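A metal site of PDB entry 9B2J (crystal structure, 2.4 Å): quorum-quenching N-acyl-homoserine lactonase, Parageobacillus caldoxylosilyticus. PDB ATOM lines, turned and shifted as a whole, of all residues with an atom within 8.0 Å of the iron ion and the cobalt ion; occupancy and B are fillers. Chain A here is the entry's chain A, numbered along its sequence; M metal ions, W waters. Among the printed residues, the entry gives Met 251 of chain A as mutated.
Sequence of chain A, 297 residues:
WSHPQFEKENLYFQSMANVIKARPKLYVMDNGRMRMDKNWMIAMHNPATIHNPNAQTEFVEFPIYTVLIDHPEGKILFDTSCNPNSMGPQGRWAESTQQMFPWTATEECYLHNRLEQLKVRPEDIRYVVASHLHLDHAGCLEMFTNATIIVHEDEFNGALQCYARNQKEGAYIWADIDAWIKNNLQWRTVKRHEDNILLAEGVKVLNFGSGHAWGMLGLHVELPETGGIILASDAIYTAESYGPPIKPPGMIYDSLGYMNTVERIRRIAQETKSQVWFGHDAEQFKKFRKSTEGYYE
The side-chain hydroxyl (OH) of Tyr 172 lies within hydrogen-bond range of a ring nitrogen (NE2) of His 134 (3.4 Å). The side-chain hydroxyl (OG) of Ser 233 lies close to a ring nitrogen (ND1) of His 137 (3.5 Å). A ring nitrogen (ND1) of His 137 is in hydrogen-bond range of the side-chain carboxylate (OD2) of Asp 79, at 2.8 Å. ND1 of His 132 lies within hydrogen-bond range of OG of Ser 131. The backbone carbonyl oxygen (O) of Met 251 sits at hydrogen-bond distance from a ring nitrogen (ND1) of His 212, 3.2 Å away. N of His 280 lies within hydrogen-bond range of O of Tyr 237 (3.0 Å). ND1 of His 280 sits at hydrogen-bond distance from O of Pro 63 (2.8 Å).
The cobalt ion is bound by a ring nitrogen (ND1) of His 134, the side-chain carboxylate of Asp 234, a ring nitrogen (NE2) of His 132, a ring nitrogen (NE2) of His 212, water W1 and water W2. The cobalt ion has six donor atoms within binding distance.
Water W1 lies within hydrogen-bond range of the side-chain hydroxyl of Tyr 237 (2.8 Å) and the side-chain sulfur of Met 251 (3.3 Å).
Four residues have an atom within 4 Å of the cobalt ion: His 132, His 134, His 212 and Asp 234.
The iron ion is bound by water W2 (2.0 Å). A ring nitrogen (NE2) of His 137 is bound to the iron ion, at 2.1 Å. OD2 of Asp 234 binds the iron ion (2.1 Å). The iron ion is bound by OD2 of Asp 136, 2.2 Å away. NE2 of His 280 binds the iron ion (2.3 Å). The iron ion has five donor atoms within binding distance. Slightly farther from the iron ion lies water W3 (2.7 Å).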
ATOM      1  N   MET A  34      10.338 -14.871  -9.197  1.00  0.00           N
ATOM      2  CA  MET A  34      10.996 -15.950  -8.464  1.00  0.00           C
ATOM      3  C   MET A  34      11.119 -17.166  -9.391  1.00  0.00           C
ATOM      4  O   MET A  34      10.283 -17.332 -10.277  1.00  0.00           O
ATOM      5  CB  MET A  34      10.189 -16.344  -7.222  1.00  0.00           C
ATOM      6  CG  MET A  34      10.753 -17.513  -6.420  1.00  0.00           C
ATOM      7  SD  MET A  34       9.885 -17.797  -4.859  1.00  0.00           S
ATOM      8  CE  MET A  34      10.349 -16.327  -3.941  1.00  0.00           C
ATOM      9  N   MET A  36      12.019 -21.621  -9.421  1.00  0.00           N
ATOM     10  CA  MET A  36      12.105 -22.830  -8.609  1.00  0.00           C
ATOM     11  C   MET A  36      11.825 -24.089  -9.453  1.00  0.00           C
ATOM     12  O   MET A  36      11.315 -23.981 -10.563  1.00  0.00           O
ATOM     13  CB  MET A  36      11.107 -22.794  -7.449  1.00  0.00           C
ATOM     14  CG  MET A  36       9.670 -23.052  -7.851  1.00  0.00           C
ATOM     15  SD  MET A  36       8.522 -22.942  -6.467  1.00  0.00           S
ATOM     16  CE  MET A  36       6.968 -23.375  -7.268  1.00  0.00           C
ATOM     17  N   PHE A  62       8.190 -17.403 -12.385  1.00  0.00           N
ATOM     18  CA  PHE A  62       6.811 -17.002 -12.129  1.00  0.00           C
ATOM     19  C   PHE A  62       6.799 -15.663 -11.395  1.00  0.00           C
ATOM     20  O   PHE A  62       7.757 -15.314 -10.719  1.00  0.00           O
ATOM     21  CB  PHE A  62       6.045 -18.076 -11.334  1.00  0.00           C
ATOM     22  CG  PHE A  62       6.683 -18.445 -10.003  1.00  0.00           C
ATOM     23  CD1 PHE A  62       6.363 -17.751  -8.838  1.00  0.00           C
ATOM     24  CD2 PHE A  62       7.602 -19.481  -9.917  1.00  0.00           C
ATOM     25  CE1 PHE A  62       6.945 -18.098  -7.633  1.00  0.00           C
ATOM     26  CE2 PHE A  62       8.184 -19.821  -8.704  1.00  0.00           C
ATOM     27  CZ  PHE A  62       7.856 -19.129  -7.562  1.00  0.00           C
ATOM     28  N   PRO A  63       5.708 -14.862 -11.514  1.00  0.00           N
ATOM     29  CA  PRO A  63       5.631 -13.545 -10.884  1.00  0.00           C
ATOM     30  C   PRO A  63       5.197 -13.559  -9.412  1.00  0.00           C
ATOM     31  O   PRO A  63       4.355 -14.363  -9.032  1.00  0.00           O
ATOM     32  CB  PRO A  63       4.584 -12.830 -11.759  1.00  0.00           C
ATOM     33  CG  PRO A  63       3.641 -13.939 -12.192  1.00  0.00           C
ATOM     34  CD  PRO A  63       4.494 -15.204 -12.284  1.00  0.00           C
ATOM     35  N   ILE A  64       5.795 -12.656  -8.618  1.00  0.00           N
ATOM     36  CA  ILE A  64       5.326 -12.308  -7.284  1.00  0.00           C
ATOM     37  C   ILE A  64       4.551 -10.988  -7.384  1.00  0.00           C
ATOM     38  O   ILE A  64       5.092 -10.008  -7.917  1.00  0.00           O
ATOM     39  CB  ILE A  64       6.513 -12.185  -6.305  1.00  0.00           C
ATOM     40  CG1 ILE A  64       7.470 -13.374  -6.381  1.00  0.00           C
ATOM     41  CG2 ILE A  64       6.027 -11.937  -4.873  1.00  0.00           C
ATOM     42  CD1 ILE A  64       6.786 -14.731  -6.237  1.00  0.00           C
ATOM     43  N   ASP A  79      -1.723  -9.528   0.442  1.00  0.00           N
ATOM     44  CA  ASP A  79      -0.346 -10.035   0.351  1.00  0.00           C
ATOM     45  C   ASP A  79       0.649  -8.886   0.407  1.00  0.00           C
ATOM     46  O   ASP A  79       0.257  -7.725   0.272  1.00  0.00           O
ATOM     47  CB  ASP A  79      -0.167 -10.961  -0.850  1.00  0.00           C
ATOM     48  CG  ASP A  79      -0.647 -12.398  -0.643  1.00  0.00           C
ATOM     49  OD1 ASP A  79      -0.931 -12.763   0.521  1.00  0.00           O
ATOM     50  OD2 ASP A  79      -0.736 -13.131  -1.654  1.00  0.00           O
ATOM     51  N   SER A 131      -2.595 -14.046   2.799  1.00  0.00           N
ATOM     52  CA  SER A 131      -3.133 -15.290   2.250  1.00  0.00           C
ATOM     53  C   SER A 131      -2.548 -16.476   3.002  1.00  0.00           C
ATOM     54  O   SER A 131      -3.278 -17.405   3.369  1.00  0.00           O
ATOM     55  CB  SER A 131      -2.902 -15.392   0.759  1.00  0.00           C
ATOM     56  OG  SER A 131      -1.517 -15.508   0.445  1.00  0.00           O
ATOM     57  N   HIS A 132      -1.225 -16.444   3.213  1.00  0.00           N
ATOM     58  CA  HIS A 132      -0.490 -17.351   4.102  1.00  0.00           C
ATOM     59  C   HIS A 132       0.833 -16.674   4.452  1.00  0.00           C
ATOM     60  O   HIS A 132       1.056 -15.525   4.043  1.00  0.00           O
ATOM     61  CB  HIS A 132      -0.381 -18.759   3.513  1.00  0.00           C
ATOM     62  CG  HIS A 132       0.296 -18.846   2.191  1.00  0.00           C
ATOM     63  ND1 HIS A 132      -0.019 -18.010   1.140  1.00  0.00           N
ATOM     64  CD2 HIS A 132       1.240 -19.680   1.735  1.00  0.00           C
ATOM     65  CE1 HIS A 132       0.726 -18.321   0.089  1.00  0.00           C
ATOM     66  NE2 HIS A 132       1.503 -19.339   0.427  1.00  0.00           N
ATOM     67  N   LEU A 133       1.724 -17.352   5.206  1.00  0.00           N
ATOM     68  CA  LEU A 133       2.891 -16.687   5.780  1.00  0.00           C
ATOM     69  C   LEU A 133       4.191 -17.204   5.168  1.00  0.00           C
ATOM     70  O   LEU A 133       5.244 -17.148   5.804  1.00  0.00           O
ATOM     71  CB  LEU A 133       2.874 -16.857   7.300  1.00  0.00           C
ATOM     72  CG  LEU A 133       1.693 -16.188   8.022  1.00  0.00           C
ATOM     73  CD1 LEU A 133       1.765 -16.377   9.528  1.00  0.00           C
ATOM     74  CD2 LEU A 133       1.622 -14.703   7.677  1.00  0.00           C
ATOM     75  N   HIS A 134       4.126 -17.651   3.900  1.00  0.00           N
ATOM     76  CA  HIS A 134       5.295 -18.023   3.113  1.00  0.00           C
ATOM     77  C   HIS A 134       6.120 -16.774   2.782  1.00  0.00           C
ATOM     78  O   HIS A 134       5.602 -15.658   2.820  1.00  0.00           O
ATOM     79  CB  HIS A 134       4.874 -18.758   1.832  1.00  0.00           C
ATOM     80  CG  HIS A 134       4.566 -20.213   2.021  1.00  0.00           C
ATOM     81  ND1 HIS A 134       3.959 -20.969   1.047  1.00  0.00           N
ATOM     82  CD2 HIS A 134       4.813 -21.041   3.045  1.00  0.00           C
ATOM     83  CE1 HIS A 134       3.840 -22.212   1.484  1.00  0.00           C
ATOM     84  NE2 HIS A 134       4.348 -22.280   2.700  1.00  0.00           N
ATOM     85  N   LEU A 135       7.400 -16.989   2.420  1.00  0.00           N
ATOM     86  CA  LEU A 135       8.409 -15.937   2.262  1.00  0.00           C
ATOM     87  C   LEU A 135       8.034 -14.945   1.162  1.00  0.00           C
ATOM     88  O   LEU A 135       8.471 -13.790   1.210  1.00  0.00           O
ATOM     89  CB  LEU A 135       9.776 -16.587   1.990  1.00  0.00           C
ATOM     90  CG  LEU A 135       9.942 -17.315   0.658  1.00  0.00           C
ATOM     91  CD1 LEU A 135      11.346 -17.868   0.513  1.00  0.00           C
ATOM     92  CD2 LEU A 135       8.921 -18.435   0.495  1.00  0.00           C
ATOM     93  N   ASP A 136       7.214 -15.360   0.183  1.00  0.00           N
ATOM     94  CA  ASP A 136       6.905 -14.555  -0.994  1.00  0.00           C
ATOM     95  C   ASP A 136       5.538 -13.870  -0.883  1.00  0.00           C
ATOM     96  O   ASP A 136       5.082 -13.271  -1.856  1.00  0.00           O
ATOM     97  CB  ASP A 136       6.979 -15.371  -2.271  1.00  0.00           C
ATOM     98  CG  ASP A 136       6.102 -16.628  -2.279  1.00  0.00           C
ATOM     99  OD1 ASP A 136       6.143 -17.367  -1.274  1.00  0.00           O
ATOM    100  OD2 ASP A 136       5.410 -16.855  -3.286  1.00  0.00           O
ATOM    101  N   HIS A 137       4.896 -13.947   0.296  1.00  0.00           N
ATOM    102  CA  HIS A 137       3.586 -13.336   0.533  1.00  0.00           C
ATOM    103  C   HIS A 137       3.585 -12.505   1.821  1.00  0.00           C
ATOM    104  O   HIS A 137       2.819 -11.547   1.921  1.00  0.00           O
ATOM    105  CB  HIS A 137       2.476 -14.388   0.571  1.00  0.00           C
ATOM    106  CG  HIS A 137       2.351 -15.209  -0.658  1.00  0.00           C
ATOM    107  ND1 HIS A 137       1.412 -14.974  -1.634  1.00  0.00           N
ATOM    108  CD2 HIS A 137       3.054 -16.280  -1.070  1.00  0.00           C
ATOM    109  CE1 HIS A 137       1.557 -15.866  -2.611  1.00  0.00           C
ATOM    110  NE2 HIS A 137       2.544 -16.677  -2.283  1.00  0.00           N
ATOM    111  N   GLU A 155      -2.216 -21.064  10.319  1.00  0.00           N
ATOM    112  CA  GLU A 155      -1.017 -20.587   9.631  1.00  0.00           C
ATOM    113  C   GLU A 155      -0.126 -19.829  10.618  1.00  0.00           C
ATOM    114  O   GLU A 155       1.090 -20.032  10.646  1.00  0.00           O
ATOM    115  CB  GLU A 155      -1.420 -19.686   8.449  1.00  0.00           C
ATOM    116  CG  GLU A 155      -0.252 -19.252   7.572  1.00  0.00           C
ATOM    117  CD  GLU A 155       0.329 -20.339   6.682  1.00  0.00           C
ATOM    118  OE1 GLU A 155      -0.251 -21.436   6.647  1.00  0.00           O
ATOM    119  OE2 GLU A 155       1.355 -20.077   6.022  1.00  0.00           O
ATOM    120  N   ALA A 171      10.197 -22.365   4.149  1.00  0.00           N
ATOM    121  CA  ALA A 171       9.426 -21.287   3.533  1.00  0.00           C
ATOM    122  C   ALA A 171       9.058 -20.198   4.549  1.00  0.00           C
ATOM    123  O   ALA A 171       8.524 -19.161   4.163  1.00  0.00           O
ATOM    124  CB  ALA A 171       8.187 -21.877   2.882  1.00  0.00           C
ATOM    125  N   TYR A 172       9.338 -20.427   5.829  1.00  0.00           N
ATOM    126  CA  TYR A 172       8.974 -19.509   6.906  1.00  0.00           C
ATOM    127  C   TYR A 172      10.238 -18.834   7.457  1.00  0.00           C
ATOM    128  O   TYR A 172      10.997 -19.457   8.190  1.00  0.00           O
ATOM    129  CB  TYR A 172       8.142 -20.258   7.950  1.00  0.00           C
ATOM    130  CG  TYR A 172       6.801 -20.734   7.419  1.00  0.00           C
ATOM    131  CD1 TYR A 172       5.700 -19.889   7.391  1.00  0.00           C
ATOM    132  CD2 TYR A 172       6.641 -22.009   6.904  1.00  0.00           C
ATOM    133  CE1 TYR A 172       4.479 -20.302   6.884  1.00  0.00           C
ATOM    134  CE2 TYR A 172       5.426 -22.446   6.401  1.00  0.00           C
ATOM    135  CZ  TYR A 172       4.345 -21.593   6.391  1.00  0.00           C
ATOM    136  OH  TYR A 172       3.144 -22.004   5.893  1.00  0.00           O
ATOM    137  N   HIS A 212      -2.497 -26.127   0.555  1.00  0.00           N
ATOM    138  CA  HIS A 212      -1.135 -25.704   0.210  1.00  0.00           C
ATOM    139  C   HIS A 212      -0.307 -25.556   1.480  1.00  0.00           C
ATOM    140  O   HIS A 212       0.808 -26.064   1.560  1.00  0.00           O
ATOM    141  CB  HIS A 212      -1.173 -24.411  -0.627  1.00  0.00           C
ATOM    142  CG  HIS A 212       0.146 -23.735  -0.796  1.00  0.00           C
ATOM    143  ND1 HIS A 212       1.192 -24.302  -1.511  1.00  0.00           N
ATOM    144  CD2 HIS A 212       0.601 -22.555  -0.346  1.00  0.00           C
ATOM    145  CE1 HIS A 212       2.234 -23.481  -1.490  1.00  0.00           C
ATOM    146  NE2 HIS A 212       1.893 -22.408  -0.798  1.00  0.00           N
ATOM    147  N   ALA A 213      -0.861 -24.832   2.471  1.00  0.00           N
ATOM    148  CA  ALA A 213      -0.229 -24.575   3.756  1.00  0.00           C
ATOM    149  C   ALA A 213      -1.214 -24.878   4.891  1.00  0.00           C
ATOM    150  O   ALA A 213      -2.258 -25.475   4.658  1.00  0.00           O
ATOM    151  CB  ALA A 213       0.265 -23.148   3.816  1.00  0.00           C
ATOM    152  N   MET A 216      -5.103 -21.181   4.556  1.00  0.00           N
ATOM    153  CA  MET A 216      -5.140 -20.267   3.412  1.00  0.00           C
ATOM    154  C   MET A 216      -6.338 -19.320   3.524  1.00  0.00           C
ATOM    155  O   MET A 216      -7.435 -19.749   3.864  1.00  0.00           O
ATOM    156  CB  MET A 216      -5.269 -21.042   2.088  1.00  0.00           C
ATOM    157  CG  MET A 216      -4.230 -22.117   1.902  1.00  0.00           C
ATOM    158  SD  MET A 216      -2.539 -21.479   1.944  1.00  0.00           S
ATOM    159  CE  MET A 216      -2.387 -20.799   0.285  1.00  0.00           C
ATOM    160  N   SER A 233      -4.588 -16.754  -4.505  1.00  0.00           N
ATOM    161  CA  SER A 233      -3.206 -16.900  -4.068  1.00  0.00           C
ATOM    162  C   SER A 233      -2.723 -18.329  -4.336  1.00  0.00           C
ATOM    163  O   SER A 233      -3.010 -18.883  -5.394  1.00  0.00           O
ATOM    164  CB  SER A 233      -3.034 -16.501  -2.622  1.00  0.00           C
ATOM    165  OG  SER A 233      -1.654 -16.474  -2.260  1.00  0.00           O
ATOM    166  N   ASP A 234      -1.989 -18.920  -3.379  1.00  0.00           N
ATOM    167  CA  ASP A 234      -1.299 -20.189  -3.584  1.00  0.00           C
ATOM    168  C   ASP A 234      -2.233 -21.381  -3.402  1.00  0.00           C
ATOM    169  O   ASP A 234      -1.778 -22.529  -3.365  1.00  0.00           O
ATOM    170  CB  ASP A 234      -0.062 -20.297  -2.712  1.00  0.00           C
ATOM    171  CG  ASP A 234       1.119 -19.461  -3.177  1.00  0.00           C
ATOM    172  OD1 ASP A 234       0.930 -18.676  -4.134  1.00  0.00           O
ATOM    173  OD2 ASP A 234       2.222 -19.614  -2.601  1.00  0.00           O
ATOM    174  N   ALA A 235      -3.544 -21.127  -3.289  1.00  0.00           N
ATOM    175  CA  ALA A 235      -4.563 -22.167  -3.325  1.00  0.00           C
ATOM    176  C   ALA A 235      -4.677 -22.740  -4.747  1.00  0.00           C
ATOM    177  O   ALA A 235      -5.042 -23.901  -4.917  1.00  0.00           O
ATOM    178  CB  ALA A 235      -5.888 -21.625  -2.841  1.00  0.00           C
ATOM    179  N   TYR A 237      -1.928 -22.267  -7.986  1.00  0.00           N
ATOM    180  CA  TYR A 237      -0.701 -21.668  -8.515  1.00  0.00           C
ATOM    181  C   TYR A 237      -0.963 -21.053  -9.903  1.00  0.00           C
ATOM    182  O   TYR A 237      -0.703 -19.866 -10.093  1.00  0.00           O
ATOM    183  CB  TYR A 237       0.415 -22.714  -8.602  1.00  0.00           C
ATOM    184  CG  TYR A 237       1.301 -22.895  -7.379  1.00  0.00           C
ATOM    185  CD1 TYR A 237       1.490 -21.874  -6.459  1.00  0.00           C
ATOM    186  CD2 TYR A 237       1.975 -24.093  -7.166  1.00  0.00           C
ATOM    187  CE1 TYR A 237       2.318 -22.040  -5.356  1.00  0.00           C
ATOM    188  CE2 TYR A 237       2.800 -24.273  -6.066  1.00  0.00           C
ATOM    189  CZ  TYR A 237       2.972 -23.246  -5.161  1.00  0.00           C
ATOM    190  OH  TYR A 237       3.789 -23.422  -4.075  1.00  0.00           O
ATOM    191  N   MET A 251       4.585 -28.741  -3.438  1.00  0.00           N
ATOM    192  CA  MET A 251       4.523 -27.987  -2.190  1.00  0.00           C
ATOM    193  C   MET A 251       3.094 -28.007  -1.664  1.00  0.00           C
ATOM    194  O   MET A 251       2.218 -27.287  -2.166  1.00  0.00           O
ATOM    195  CB  MET A 251       5.010 -26.544  -2.352  1.00  0.00           C
ATOM    196  CG  MET A 251       5.228 -25.835  -1.021  1.00  0.00           C
ATOM    197  SD  MET A 251       6.021 -24.218  -1.172  1.00  0.00           S
ATOM    198  CE  MET A 251       7.438 -24.642  -2.203  1.00  0.00           C
ATOM    199  N   GLY A 279      -2.163 -17.467  -8.194  1.00  0.00           N
ATOM    200  CA  GLY A 279      -1.096 -16.988  -7.321  1.00  0.00           C
ATOM    201  C   GLY A 279       0.153 -16.562  -8.097  1.00  0.00           C
ATOM    202  O   GLY A 279       0.778 -15.567  -7.754  1.00  0.00           O
ATOM    203  N   HIS A 280       0.488 -17.336  -9.142  1.00  0.00           N
ATOM    204  CA  HIS A 280       1.793 -17.275  -9.792  1.00  0.00           C
ATOM    205  C   HIS A 280       1.715 -17.723 -11.255  1.00  0.00           C
ATOM    206  O   HIS A 280       2.570 -18.478 -11.704  1.00  0.00           O
ATOM    207  CB  HIS A 280       2.790 -18.158  -9.040  1.00  0.00           C
ATOM    208  CG  HIS A 280       3.064 -17.724  -7.635  1.00  0.00           C
ATOM    209  ND1 HIS A 280       3.574 -16.486  -7.328  1.00  0.00           N
ATOM    210  CD2 HIS A 280       2.942 -18.372  -6.456  1.00  0.00           C
ATOM    211  CE1 HIS A 280       3.736 -16.383  -6.013  1.00  0.00           C
ATOM    212  NE2 HIS A 280       3.350 -17.521  -5.470  1.00  0.00           N
HETATM  213 FE    FE M   1       3.672 -18.174  -3.254  1.00  0.00          FE
HETATM  214 CO    CO M   2       3.012 -20.464  -0.754  1.00  0.00          CO
HETATM  215  O   HOH W   1       4.517 -21.411  -2.211  1.00  0.00           O
HETATM  216  O   HOH W   2       4.685 -19.165  -1.783  1.00  0.00           O
HETATM  217  O   HOH W   3       5.407 -20.183  -3.840  1.00  0.00           O
